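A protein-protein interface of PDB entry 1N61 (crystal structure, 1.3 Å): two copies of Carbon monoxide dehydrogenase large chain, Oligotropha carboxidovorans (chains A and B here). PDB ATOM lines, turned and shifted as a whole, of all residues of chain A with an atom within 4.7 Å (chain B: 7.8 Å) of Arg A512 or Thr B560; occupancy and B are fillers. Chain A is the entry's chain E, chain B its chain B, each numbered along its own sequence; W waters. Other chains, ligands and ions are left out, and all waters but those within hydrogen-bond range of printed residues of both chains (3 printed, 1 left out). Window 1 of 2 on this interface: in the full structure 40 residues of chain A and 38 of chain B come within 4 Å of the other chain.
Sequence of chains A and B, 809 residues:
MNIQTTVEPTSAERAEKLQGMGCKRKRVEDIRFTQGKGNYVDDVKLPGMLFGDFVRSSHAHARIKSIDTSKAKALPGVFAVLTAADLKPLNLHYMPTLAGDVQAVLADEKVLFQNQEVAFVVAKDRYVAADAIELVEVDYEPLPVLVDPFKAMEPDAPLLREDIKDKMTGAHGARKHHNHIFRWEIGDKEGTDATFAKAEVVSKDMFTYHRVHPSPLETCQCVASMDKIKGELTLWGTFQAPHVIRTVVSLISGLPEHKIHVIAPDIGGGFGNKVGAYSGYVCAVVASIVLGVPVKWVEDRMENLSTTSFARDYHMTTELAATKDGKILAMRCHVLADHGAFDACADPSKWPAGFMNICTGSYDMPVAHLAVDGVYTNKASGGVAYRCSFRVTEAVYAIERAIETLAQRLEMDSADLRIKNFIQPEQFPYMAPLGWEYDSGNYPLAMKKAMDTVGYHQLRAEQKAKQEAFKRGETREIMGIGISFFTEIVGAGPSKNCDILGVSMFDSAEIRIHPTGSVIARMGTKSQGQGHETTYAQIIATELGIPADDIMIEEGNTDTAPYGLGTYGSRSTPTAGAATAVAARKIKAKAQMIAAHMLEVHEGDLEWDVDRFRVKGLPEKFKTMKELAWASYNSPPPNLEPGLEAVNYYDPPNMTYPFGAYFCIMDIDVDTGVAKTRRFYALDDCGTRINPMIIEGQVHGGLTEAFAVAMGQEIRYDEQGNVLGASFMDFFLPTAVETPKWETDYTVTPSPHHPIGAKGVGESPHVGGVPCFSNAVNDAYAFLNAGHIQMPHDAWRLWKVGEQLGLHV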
ATOM      1  N   GLU A 510      23.699   4.162 -28.223  1.00  0.00           N
ATOM      2  CA  GLU A 510      23.564   3.249 -27.102  1.00  0.00           C
ATOM      3  C   GLU A 510      22.136   2.763 -27.096  1.00  0.00           C
ATOM      4  O   GLU A 510      21.224   3.544 -27.097  1.00  0.00           O
ATOM      5  CB  GLU A 510      23.932   3.932 -25.768  1.00  0.00           C
ATOM      6  CG  GLU A 510      23.789   2.952 -24.594  1.00  0.00           C
ATOM      7  CD  GLU A 510      24.536   3.333 -23.338  1.00  0.00           C
ATOM      8  OE1 GLU A 510      24.710   4.545 -23.076  1.00  0.00           O
ATOM      9  OE2 GLU A 510      24.970   2.402 -22.591  1.00  0.00           O
ATOM     10  N   ILE A 511      21.990   1.455 -27.043  1.00  0.00           N
ATOM     11  CA  ILE A 511      20.672   0.808 -27.104  1.00  0.00           C
ATOM     12  C   ILE A 511      20.529  -0.157 -25.929  1.00  0.00           C
ATOM     13  O   ILE A 511      21.389  -1.004 -25.742  1.00  0.00           O
ATOM     14  CB  ILE A 511      20.508   0.049 -28.406  1.00  0.00           C
ATOM     15  CG1 ILE A 511      20.704   0.943 -29.647  1.00  0.00           C
ATOM     16  CG2 ILE A 511      19.115  -0.633 -28.453  1.00  0.00           C
ATOM     17  CD1 ILE A 511      20.692   0.131 -30.973  1.00  0.00           C
ATOM     18  N   ARG A 512      19.454  -0.022 -25.146  1.00  0.00           N
ATOM     19  CA  ARG A 512      19.220  -0.884 -23.992  1.00  0.00           C
ATOM     20  C   ARG A 512      17.823  -1.446 -24.071  1.00  0.00           C
ATOM     21  O   ARG A 512      16.838  -0.696 -24.171  1.00  0.00           O
ATOM     22  CB  ARG A 512      19.410  -0.074 -22.691  1.00  0.00           C
ATOM     23  CG  ARG A 512      19.014  -0.770 -21.404  1.00  0.00           C
ATOM     24  CD  ARG A 512      19.363   0.039 -20.167  1.00  0.00           C
ATOM     25  NE  ARG A 512      20.792   0.133 -19.990  1.00  0.00           N
ATOM     26  CZ  ARG A 512      21.494   1.257 -19.922  1.00  0.00           C
ATOM     27  NH1 ARG A 512      20.902   2.402 -19.605  1.00  0.00           N
ATOM     28  NH2 ARG A 512      22.819   1.172 -19.897  1.00  0.00           N
ATOM     29  N   ILE A 513      17.744  -2.778 -24.026  1.00  0.00           N
ATOM     30  CA  ILE A 513      16.473  -3.477 -24.085  1.00  0.00           C
ATOM     31  C   ILE A 513      16.048  -3.844 -22.667  1.00  0.00           C
ATOM     32  O   ILE A 513      16.808  -4.438 -21.894  1.00  0.00           O
ATOM     33  CB  ILE A 513      16.586  -4.772 -24.927  1.00  0.00           C
ATOM     34  CG1 ILE A 513      17.512  -4.580 -26.144  1.00  0.00           C
ATOM     35  CG2 ILE A 513      15.206  -5.289 -25.285  1.00  0.00           C
ATOM     36  CD1 ILE A 513      16.984  -3.723 -27.250  1.00  0.00           C
ATOM     37  N   HIS A 514      14.844  -3.456 -22.308  1.00  0.00           N
ATOM     38  CA  HIS A 514      14.259  -3.730 -21.007  1.00  0.00           C
ATOM     39  C   HIS A 514      13.752  -5.190 -20.907  1.00  0.00           C
ATOM     40  O   HIS A 514      13.595  -5.888 -21.923  1.00  0.00           O
ATOM     41  CB  HIS A 514      13.095  -2.755 -20.784  1.00  0.00           C
ATOM     42  CG  HIS A 514      13.517  -1.344 -20.754  1.00  0.00           C
ATOM     43  ND1 HIS A 514      14.725  -0.965 -20.197  1.00  0.00           N
ATOM     44  CD2 HIS A 514      12.931  -0.221 -21.242  1.00  0.00           C
ATOM     45  CE1 HIS A 514      14.823   0.354 -20.315  1.00  0.00           C
ATOM     46  NE2 HIS A 514      13.746   0.822 -20.902  1.00  0.00           N
ATOM     47  N   SER A 518      10.734  -3.572 -24.486  1.00  0.00           N
ATOM     48  CA  SER A 518      10.852  -2.221 -24.961  1.00  0.00           C
ATOM     49  C   SER A 518      12.257  -1.709 -24.795  1.00  0.00           C
ATOM     50  O   SER A 518      13.127  -2.413 -24.244  1.00  0.00           O
ATOM     51  CB  SER A 518       9.819  -1.309 -24.257  1.00  0.00           C
ATOM     52  OG  SER A 518       9.997  -1.358 -22.852  1.00  0.00           O
ATOM     53  N   VAL A 519      12.532  -0.553 -25.388  1.00  0.00           N
ATOM     54  CA  VAL A 519      13.909  -0.120 -25.632  1.00  0.00           C
ATOM     55  C   VAL A 519      14.071   1.361 -25.326  1.00  0.00           C
ATOM     56  O   VAL A 519      13.186   2.149 -25.696  1.00  0.00           O
ATOM     57  CB  VAL A 519      14.228  -0.330 -27.060  1.00  0.00           C
ATOM     58  CG1 VAL A 519      15.665   0.125 -27.373  1.00  0.00           C
ATOM     59  CG2 VAL A 519      13.978  -1.767 -27.442  1.00  0.00           C
ATOM     60  N   ILE A 520      15.186   1.748 -24.712  1.00  0.00           N
ATOM     61  CA  ILE A 520      15.622   3.137 -24.695  1.00  0.00           C
ATOM     62  C   ILE A 520      16.943   3.200 -25.478  1.00  0.00           C
ATOM     63  O   ILE A 520      17.858   2.396 -25.224  1.00  0.00           O
ATOM     64  CB  ILE A 520      15.773   3.676 -23.222  1.00  0.00           C
ATOM     65  CG1 ILE A 520      16.375   5.076 -23.193  1.00  0.00           C
ATOM     66  CG2 ILE A 520      16.672   2.795 -22.377  1.00  0.00           C
ATOM     67  CD1 ILE A 520      15.536   6.132 -23.812  1.00  0.00           C
ATOM     68  N   ARG A 522      19.830   6.112 -27.266  1.00  0.00           N
ATOM     69  CA  ARG A 522      20.288   7.484 -27.341  1.00  0.00           C
ATOM     70  C   ARG A 522      21.450   7.554 -28.340  1.00  0.00           C
ATOM     71  O   ARG A 522      22.192   6.607 -28.499  1.00  0.00           O
ATOM     72  CB  ARG A 522      20.741   7.993 -25.961  1.00  0.00           C
ATOM     73  CG  ARG A 522      19.713   7.881 -24.888  1.00  0.00           C
ATOM     74  CD  ARG A 522      20.034   8.727 -23.708  1.00  0.00           C
ATOM     75  NE  ARG A 522      18.965   8.739 -22.740  1.00  0.00           N
ATOM     76  CZ  ARG A 522      18.766   7.789 -21.841  1.00  0.00           C
ATOM     77  NH1 ARG A 522      19.698   6.878 -21.630  1.00  0.00           N
ATOM     78  NH2 ARG A 522      17.770   7.912 -20.967  1.00  0.00           N
ATOM     79  N   THR A 560      23.462  12.025 -20.434  1.00  0.00           N
ATOM     80  CA  THR A 560      22.855  10.736 -20.706  1.00  0.00           C
ATOM     81  C   THR A 560      23.200  10.149 -22.084  1.00  0.00           C
ATOM     82  O   THR A 560      23.352   8.930 -22.224  1.00  0.00           O
ATOM     83  CB  THR A 560      21.338  10.784 -20.512  1.00  0.00           C
ATOM     84  OG1 THR A 560      20.718  11.609 -21.521  1.00  0.00           O
ATOM     85  CG2 THR A 560      20.944  11.371 -19.124  1.00  0.00           C
ATOM     86  N   LEU A 644      20.731  -7.001 -21.959  1.00  0.00           N
ATOM     87  CA  LEU A 644      20.762  -7.010 -23.390  1.00  0.00           C
ATOM     88  C   LEU A 644      20.829  -5.560 -23.858  1.00  0.00           C
ATOM     89  O   LEU A 644      19.808  -4.860 -23.953  1.00  0.00           O
ATOM     90  CB  LEU A 644      19.592  -7.776 -23.952  1.00  0.00           C
ATOM     91  CG  LEU A 644      19.679  -8.045 -25.426  1.00  0.00           C
ATOM     92  CD1 LEU A 644      20.926  -8.863 -25.803  1.00  0.00           C
ATOM     93  CD2 LEU A 644      18.418  -8.777 -25.874  1.00  0.00           C
ATOM     94  N   GLU A 645      22.042  -5.090 -24.114  1.00  0.00           N
ATOM     95  CA  GLU A 645      22.305  -3.720 -24.475  1.00  0.00           C
ATOM     96  C   GLU A 645      23.637  -3.633 -25.200  1.00  0.00           C
ATOM     97  O   GLU A 645      24.464  -4.528 -25.116  1.00  0.00           O
ATOM     98  CB  GLU A 645      22.266  -2.826 -23.261  1.00  0.00           C
ATOM     99  CG  GLU A 645      23.304  -3.143 -22.208  1.00  0.00           C
ATOM    100  CD  GLU A 645      23.119  -2.224 -21.027  1.00  0.00           C
ATOM    101  OE1 GLU A 645      23.909  -1.275 -20.871  1.00  0.00           O
ATOM    102  OE2 GLU A 645      22.090  -2.367 -20.318  1.00  0.00           O
ATOM    103  N   HIS B 243      14.144   0.084 -10.434  1.00  0.00           N
ATOM    104  CA  HIS B 243      13.916  -0.681 -11.665  1.00  0.00           C
ATOM    105  C   HIS B 243      12.870  -1.763 -11.464  1.00  0.00           C
ATOM    106  O   HIS B 243      12.039  -2.002 -12.339  1.00  0.00           O
ATOM    107  CB  HIS B 243      15.217  -1.246 -12.301  1.00  0.00           C
ATOM    108  CG  HIS B 243      16.221  -0.193 -12.733  1.00  0.00           C
ATOM    109  ND1 HIS B 243      17.033   0.431 -11.813  1.00  0.00           N
ATOM    110  CD2 HIS B 243      16.539   0.352 -13.952  1.00  0.00           C
ATOM    111  CE1 HIS B 243      17.814   1.288 -12.437  1.00  0.00           C
ATOM    112  NE2 HIS B 243      17.586   1.203 -13.731  1.00  0.00           N
ATOM    113  N   ARG B 246       9.593  -0.117 -11.590  1.00  0.00           N
ATOM    114  CA  ARG B 246       9.194   0.116 -12.973  1.00  0.00           C
ATOM    115  C   ARG B 246       8.573  -1.124 -13.575  1.00  0.00           C
ATOM    116  O   ARG B 246       7.551  -1.061 -14.255  1.00  0.00           O
ATOM    117  CB  ARG B 246      10.378   0.650 -13.832  1.00  0.00           C
ATOM    118  CG  ARG B 246       9.948   1.065 -15.207  1.00  0.00           C
ATOM    119  CD  ARG B 246      11.067   1.356 -16.171  1.00  0.00           C
ATOM    120  NE  ARG B 246      11.807   0.142 -16.493  1.00  0.00           N
ATOM    121  CZ  ARG B 246      13.036   0.115 -16.952  1.00  0.00           C
ATOM    122  NH1 ARG B 246      13.741   1.224 -17.162  1.00  0.00           N
ATOM    123  NH2 ARG B 246      13.600  -1.060 -17.190  1.00  0.00           N
ATOM    124  N   HIS B 258       9.562   1.605 -21.413  1.00  0.00           N
ATOM    125  CA  HIS B 258      10.197   2.798 -21.951  1.00  0.00           C
ATOM    126  C   HIS B 258       9.335   4.041 -21.775  1.00  0.00           C
ATOM    127  O   HIS B 258       9.808   5.136 -22.064  1.00  0.00           O
ATOM    128  CB  HIS B 258      10.603   2.613 -23.425  1.00  0.00           C
ATOM    129  CG  HIS B 258       9.448   2.441 -24.335  1.00  0.00           C
ATOM    130  ND1 HIS B 258       9.295   3.052 -25.573  1.00  0.00           N
ATOM    131  CD2 HIS B 258       8.395   1.637 -24.192  1.00  0.00           C
ATOM    132  CE1 HIS B 258       8.143   2.653 -26.107  1.00  0.00           C
ATOM    133  NE2 HIS B 258       7.620   1.748 -25.310  1.00  0.00           N
ATOM    134  N   VAL B 262      10.674   5.980 -13.732  1.00  0.00           N
ATOM    135  CA  VAL B 262      10.717   5.982 -12.282  1.00  0.00           C
ATOM    136  C   VAL B 262      11.950   6.729 -11.802  1.00  0.00           C
ATOM    137  O   VAL B 262      13.031   6.593 -12.356  1.00  0.00           O
ATOM    138  CB  VAL B 262      10.770   4.542 -11.736  1.00  0.00           C
ATOM    139  CG1 VAL B 262      11.032   4.499 -10.227  1.00  0.00           C
ATOM    140  CG2 VAL B 262       9.508   3.790 -12.060  1.00  0.00           C
ATOM    141  N   SER B 508      24.691  -3.915 -11.528  1.00  0.00           N
ATOM    142  CA  SER B 508      25.289  -3.382 -12.719  1.00  0.00           C
ATOM    143  C   SER B 508      25.944  -2.062 -12.494  1.00  0.00           C
ATOM    144  O   SER B 508      25.568  -1.305 -11.603  1.00  0.00           O
ATOM    145  CB  SER B 508      24.196  -3.230 -13.800  1.00  0.00           C
ATOM    146  OG  SER B 508      23.212  -2.313 -13.331  1.00  0.00           O
ATOM    147  N   ALA B 509      26.814  -1.716 -13.435  1.00  0.00           N
ATOM    148  CA  ALA B 509      27.512  -0.429 -13.459  1.00  0.00           C
ATOM    149  C   ALA B 509      27.783  -0.049 -14.909  1.00  0.00           C
ATOM    150  O   ALA B 509      28.191  -0.888 -15.708  1.00  0.00           O
ATOM    151  CB  ALA B 509      28.787  -0.510 -12.700  1.00  0.00           C
ATOM    152  N   GLU B 510      27.712   1.268 -15.173  1.00  0.00           N
ATOM    153  CA  GLU B 510      28.118   1.801 -16.473  1.00  0.00           C
ATOM    154  C   GLU B 510      29.017   3.001 -16.156  1.00  0.00           C
ATOM    155  O   GLU B 510      28.650   3.861 -15.338  1.00  0.00           O
ATOM    156  CB  GLU B 510      26.885   2.256 -17.270  1.00  0.00           C
ATOM    157  CG  GLU B 510      27.310   2.832 -18.610  1.00  0.00           C
ATOM    158  CD  GLU B 510      26.248   2.912 -19.683  1.00  0.00           C
ATOM    159  OE1 GLU B 510      25.076   3.062 -19.340  1.00  0.00           O
ATOM    160  OE2 GLU B 510      26.622   2.848 -20.878  1.00  0.00           O
ATOM    161  N   ARG B 512      31.516   6.017 -17.944  1.00  0.00           N
ATOM    162  CA  ARG B 512      31.869   6.731 -19.179  1.00  0.00           C
ATOM    163  C   ARG B 512      32.906   7.812 -18.851  1.00  0.00           C
ATOM    164  O   ARG B 512      32.652   8.665 -17.999  1.00  0.00           O
ATOM    165  CB  ARG B 512      30.604   7.347 -19.813  1.00  0.00           C
ATOM    166  CG  ARG B 512      30.856   8.165 -21.053  1.00  0.00           C
ATOM    167  CD  ARG B 512      29.569   8.634 -21.692  1.00  0.00           C
ATOM    168  NE  ARG B 512      28.929   7.522 -22.374  1.00  0.00           N
ATOM    169  CZ  ARG B 512      27.682   7.136 -22.209  1.00  0.00           C
ATOM    170  NH1 ARG B 512      26.805   7.885 -21.545  1.00  0.00           N
ATOM    171  NH2 ARG B 512      27.322   5.942 -22.672  1.00  0.00           N
ATOM    172  N   ALA B 521      29.298   7.890 -13.960  1.00  0.00           N
ATOM    173  CA  ALA B 521      29.063   6.467 -13.704  1.00  0.00           C
ATOM    174  C   ALA B 521      27.732   6.290 -12.987  1.00  0.00           C
ATOM    175  O   ALA B 521      27.358   7.083 -12.127  1.00  0.00           O
ATOM    176  CB  ALA B 521      30.191   5.855 -12.857  1.00  0.00           C
ATOM    177  N   ARG B 522      27.024   5.235 -13.374  1.00  0.00           N
ATOM    178  CA  ARG B 522      25.717   4.911 -12.799  1.00  0.00           C
ATOM    179  C   ARG B 522      25.672   3.420 -12.476  1.00  0.00           C
ATOM    180  O   ARG B 522      26.308   2.599 -13.111  1.00  0.00           O
ATOM    181  CB  ARG B 522      24.573   5.268 -13.731  1.00  0.00           C
ATOM    182  CG  ARG B 522      24.602   6.753 -14.189  1.00  0.00           C
ATOM    183  CD  ARG B 522      23.324   7.168 -14.817  1.00  0.00           C
ATOM    184  NE  ARG B 522      23.308   8.584 -15.124  1.00  0.00           N
ATOM    185  CZ  ARG B 522      23.717   9.105 -16.265  1.00  0.00           C
ATOM    186  NH1 ARG B 522      24.202   8.343 -17.243  1.00  0.00           N
ATOM    187  NH2 ARG B 522      23.627  10.424 -16.428  1.00  0.00           N
ATOM    188  N   MET B 523      24.824   3.135 -11.486  1.00  0.00           N
ATOM    189  CA  MET B 523      24.714   1.786 -10.986  1.00  0.00           C
ATOM    190  C   MET B 523      23.248   1.443 -10.825  1.00  0.00           C
ATOM    191  O   MET B 523      22.429   2.331 -10.670  1.00  0.00           O
ATOM    192  CB  MET B 523      25.447   1.597  -9.639  1.00  0.00           C
ATOM    193  CG  MET B 523      26.996   1.709  -9.750  1.00  0.00           C
ATOM    194  SD  MET B 523      27.595   3.391  -9.944  1.00  0.00           S
ATOM    195  CE  MET B 523      29.268   3.034 -10.327  1.00  0.00           C
ATOM    196  N   GLU B 554      25.689   8.383 -10.057  1.00  0.00           N
ATOM    197  CA  GLU B 554      24.218   8.495 -10.004  1.00  0.00           C
ATOM    198  C   GLU B 554      23.544   7.144  -9.899  1.00  0.00           C
ATOM    199  O   GLU B 554      24.014   6.147 -10.448  1.00  0.00           O
ATOM    200  CB  GLU B 554      23.656   9.257 -11.223  1.00  0.00           C
ATOM    201  CG  GLU B 554      24.172  10.686 -11.357  1.00  0.00           C
ATOM    202  CD  GLU B 554      23.532  11.431 -12.506  1.00  0.00           C
ATOM    203  OE1 GLU B 554      22.885  10.796 -13.364  1.00  0.00           O
ATOM    204  OE2 GLU B 554      23.605  12.686 -12.473  1.00  0.00           O
ATOM    205  N   GLU B 555      22.413   7.158  -9.212  1.00  0.00           N
ATOM    206  CA  GLU B 555      21.516   6.025  -9.081  1.00  0.00           C
ATOM    207  C   GLU B 555      20.089   6.529  -9.083  1.00  0.00           C
ATOM    208  O   GLU B 555      19.813   7.612  -8.584  1.00  0.00           O
ATOM    209  CB  GLU B 555      21.674   5.337  -7.740  1.00  0.00           C
ATOM    210  CG  GLU B 555      23.016   4.732  -7.444  1.00  0.00           C
ATOM    211  CD  GLU B 555      23.131   4.351  -5.963  1.00  0.00           C
ATOM    212  OE1 GLU B 555      22.779   5.160  -5.093  1.00  0.00           O
ATOM    213  OE2 GLU B 555      23.455   3.215  -5.616  1.00  0.00           O
ATOM    214  N   GLY B 556      19.168   5.659  -9.466  1.00  0.00           N
ATOM    215  CA  GLY B 556      17.770   5.848  -9.157  1.00  0.00           C
ATOM    216  C   GLY B 556      16.840   6.375 -10.226  1.00  0.00           C
ATOM    217  O   GLY B 556      15.618   6.298 -10.038  1.00  0.00           O
ATOM    218  N   ASN B 557      17.396   6.706 -11.380  1.00  0.00           N
ATOM    219  CA  ASN B 557      16.554   7.170 -12.489  1.00  0.00           C
ATOM    220  C   ASN B 557      16.580   6.001 -13.479  1.00  0.00           C
ATOM    221  O   ASN B 557      17.616   5.680 -14.072  1.00  0.00           O
ATOM    222  CB  ASN B 557      17.124   8.459 -13.079  1.00  0.00           C
ATOM    223  CG  ASN B 557      16.328   9.006 -14.229  1.00  0.00           C
ATOM    224  OD1 ASN B 557      15.797   8.231 -15.043  1.00  0.00           O
ATOM    225  ND2 ASN B 557      15.988  10.280 -14.130  1.00  0.00           N
ATOM    226  N   THR B 558      15.448   5.342 -13.654  1.00  0.00           N
ATOM    227  CA  THR B 558      15.415   4.113 -14.423  1.00  0.00           C
ATOM    228  C   THR B 558      15.593   4.345 -15.918  1.00  0.00           C
ATOM    229  O   THR B 558      15.959   3.446 -16.630  1.00  0.00           O
ATOM    230  CB  THR B 558      14.135   3.306 -14.176  1.00  0.00           C
ATOM    231  OG1 THR B 558      12.968   4.054 -14.573  1.00  0.00           O
ATOM    232  CG2 THR B 558      14.002   2.920 -12.736  1.00  0.00           C
ATOM    233  N   ASP B 559      15.445   5.587 -16.375  1.00  0.00           N
ATOM    234  CA  ASP B 559      15.741   5.896 -17.768  1.00  0.00           C
ATOM    235  C   ASP B 559      17.256   5.859 -18.016  1.00  0.00           C
ATOM    236  O   ASP B 559      17.679   5.612 -19.137  1.00  0.00           O
ATOM    237  CB  ASP B 559      15.287   7.321 -18.111  1.00  0.00           C
ATOM    238  CG  ASP B 559      13.813   7.501 -18.321  1.00  0.00           C
ATOM    239  OD1 ASP B 559      12.984   6.585 -18.317  1.00  0.00           O
ATOM    240  OD2 ASP B 559      13.405   8.664 -18.542  1.00  0.00           O
ATOM    241  N   THR B 560      18.050   6.196 -16.986  1.00  0.00           N
ATOM    242  CA  THR B 560      19.480   6.423 -17.176  1.00  0.00           C
ATOM    243  C   THR B 560      20.413   5.400 -16.559  1.00  0.00           C
ATOM    244  O   THR B 560      21.433   5.052 -17.119  1.00  0.00           O
ATOM    245  CB  THR B 560      19.875   7.829 -16.693  1.00  0.00           C
ATOM    246  OG1 THR B 560      19.778   7.926 -15.264  1.00  0.00           O
ATOM    247  CG2 THR B 560      18.955   8.960 -17.248  1.00  0.00           C
ATOM    248  N   ALA B 561      20.072   4.930 -15.366  1.00  0.00           N
ATOM    249  CA  ALA B 561      20.944   3.952 -14.689  1.00  0.00           C
ATOM    250  C   ALA B 561      20.752   2.590 -15.339  1.00  0.00           C
ATOM    251  O   ALA B 561      19.648   2.258 -15.804  1.00  0.00           O
ATOM    252  CB  ALA B 561      20.584   3.906 -13.228  1.00  0.00           C
ATOM    253  N   PRO B 562      21.805   1.785 -15.431  1.00  0.00           N
ATOM    254  CA  PRO B 562      21.645   0.440 -15.952  1.00  0.00           C
ATOM    255  C   PRO B 562      20.700  -0.340 -15.050  1.00  0.00           C
ATOM    256  O   PRO B 562      20.564   0.011 -13.887  1.00  0.00           O
ATOM    257  CB  PRO B 562      23.072  -0.125 -15.922  1.00  0.00           C
ATOM    258  CG  PRO B 562      23.730   0.600 -14.774  1.00  0.00           C
ATOM    259  CD  PRO B 562      23.104   1.987 -14.804  1.00  0.00           C
ATOM    260  N   TYR B 563      20.040  -1.352 -15.597  1.00  0.00           N
ATOM    261  CA  TYR B 563      19.080  -2.099 -14.802  1.00  0.00           C
ATOM    262  C   TYR B 563      19.800  -2.762 -13.647  1.00  0.00           C
ATOM    263  O   TYR B 563      20.794  -3.412 -13.851  1.00  0.00           O
ATOM    264  CB  TYR B 563      18.372  -3.137 -15.655  1.00  0.00           C
ATOM    265  CG  TYR B 563      17.087  -3.685 -15.082  1.00  0.00           C
ATOM    266  CD1 TYR B 563      17.088  -4.594 -14.032  1.00  0.00           C
ATOM    267  CD2 TYR B 563      15.866  -3.248 -15.525  1.00  0.00           C
ATOM    268  CE1 TYR B 563      15.896  -5.049 -13.498  1.00  0.00           C
ATOM    269  CE2 TYR B 563      14.708  -3.708 -14.979  1.00  0.00           C
ATOM    270  CZ  TYR B 563      14.714  -4.586 -13.978  1.00  0.00           C
ATOM    271  OH  TYR B 563      13.532  -5.009 -13.359  1.00  0.00           O
ATOM    272  N   VAL B 647      30.336  -1.144 -19.571  1.00  0.00           N
ATOM    273  CA  VAL B 647      29.263  -1.586 -18.719  1.00  0.00           C
ATOM    274  C   VAL B 647      29.594  -2.982 -18.237  1.00  0.00           C
ATOM    275  O   VAL B 647      30.232  -3.777 -18.963  1.00  0.00           O
ATOM    276  CB  VAL B 647      27.955  -1.621 -19.523  1.00  0.00           C
ATOM    277  CG1 VAL B 647      26.846  -2.123 -18.687  1.00  0.00           C
ATOM    278  CG2 VAL B 647      27.606  -0.317 -20.042  1.00  0.00           C
ATOM    279  N   TYR B 649      27.247  -6.108 -16.136  1.00  0.00           N
ATOM    280  CA  TYR B 649      26.161  -6.718 -15.336  1.00  0.00           C
ATOM    281  C   TYR B 649      26.751  -7.941 -14.692  1.00  0.00           C
ATOM    282  O   TYR B 649      27.178  -8.856 -15.361  1.00  0.00           O
ATOM    283  CB  TYR B 649      25.000  -7.089 -16.220  1.00  0.00           C
ATOM    284  CG  TYR B 649      24.096  -5.933 -16.661  1.00  0.00           C
ATOM    285  CD1 TYR B 649      24.586  -4.796 -17.261  1.00  0.00           C
ATOM    286  CD2 TYR B 649      22.748  -5.993 -16.453  1.00  0.00           C
ATOM    287  CE1 TYR B 649      23.701  -3.758 -17.661  1.00  0.00           C
ATOM    288  CE2 TYR B 649      21.887  -4.960 -16.828  1.00  0.00           C
ATOM    289  CZ  TYR B 649      22.376  -3.867 -17.421  1.00  0.00           C
ATOM    290  OH  TYR B 649      21.506  -2.866 -17.814  1.00  0.00           O
HETATM  291  O   HOH W   1      24.290   6.754 -20.409  1.00  0.00           O
HETATM  292  O   HOH W   2      22.147   5.055 -19.957  1.00  0.00           O
HETATM  293  O   HOH W   3      20.364  -4.633 -20.410  1.00  0.00           O
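Arg A512 touches Thr B560 (NH1 to O, 3.7 Å).
NE of Arg A512 touches OH of Tyr B649 (3.8 Å).
His A514 touches His B258 (CD2 to N, 3.8 Å).
CB of His B258 touches O of Val A519, at 3.5 Å.
Arg B512 touches Thr A560.
Thr A560 touches Arg B522 (CG2 to NH2, 3.9 Å).
OE1 of Glu A645 touches CG1 of Val B647 (3.8 Å).
Water W2 lies within hydrogen-bond range of the backbone carbonyl oxygen (O) of Thr B560 (2.9 Å), the guanidinium group (NH1) of Arg A512 (3.0 Å) and the guanidinium group (NH1) of Arg A522 (3.5 Å).
The guanidinium group (NE) of Arg B522 is in salt-bridge range of the side-chain carboxylate (OE1) of Glu B554 (2.9 Å).
The side-chain hydroxyl (OG1) of Thr B560 is in hydrogen-bond range of the backbone carbonyl oxygen (O) of Asn B557 (3.3 Å).
Printed residues of chain A that touch a printed residue of chain B: Glu A510, Arg A512, His A514, Ser A518, Val A519, Arg A522, Thr A560 and Glu A645.
Hydrophobic or aromatic side chains of chain A that line the printed part of chain B: His A514.
Printed residues of chain B that touch a printed residue of chain A: Arg B246, His B258, Glu B510, Arg B512, Arg B522, Asp B559, Thr B560, Val B647 and Tyr B649.
Hydrophobic or aromatic side chains of chain B within 4 Å of the printed part of chain A: His B258, Val B647 and Tyr B649.
Among the printed residues, Asp or Glu carboxylates within 4 Å of a Lys or Arg side-chain nitrogen of the other chain: Glu A510 with Arg B512 (3.0 Å) and Arg A512 with Glu B510 (3.0 Å).
Printed residues of chain A within 4 Å of Val B647: Glu A645.
Of the printed residues of chain A, Arg B512 touches Glu A510 and Thr A560.
Printed residues of chain B within 4 Å of Glu A510: Glu B510 (2.4 Å) and Arg B512 (3.0 Å).
The nearest printed residue of chain A that does not touch Arg B522 is Arg A522 (6.5 Å).
The side-chain hydroxyl (OH) of Tyr B649 lies within hydrogen-bond range of the side-chain carboxylate (OE2) of Glu A645 (2.6 Å).
ND1 of His A514 is in hydrogen-bond range of NH2 of Arg B246, 3.2 Å away.
The guanidinium group (NH2) of Arg A522 is in hydrogen-bond range of the backbone carbonyl oxygen (O) of Asp B559.
N of His B258 sits at hydrogen-bond distance from OG of Ser A518 (3.3 Å).
OE2 of Glu B510 lies close to OE2 of Glu A510 (2.4 Å).
OE1 of Glu A510 lies within salt-bridge range of NH2 of Arg B512 (3.0 Å).
The guanidinium group (NH2) of Arg A512 lies within salt-bridge range of the side-chain carboxylate (OE1) of Glu B510 (3.0 Å).
Glu A510 touches its own counterpart, Glu B510.
Glu A510 touches Arg B512, and with the chains exchanged Arg A512 touches Glu B510.
Thr A560 touches Arg B522, but with the chains exchanged Arg A522 does not touch Thr B560 (4.04 Å).
Thr A560 touches its own counterpart, Thr B560.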
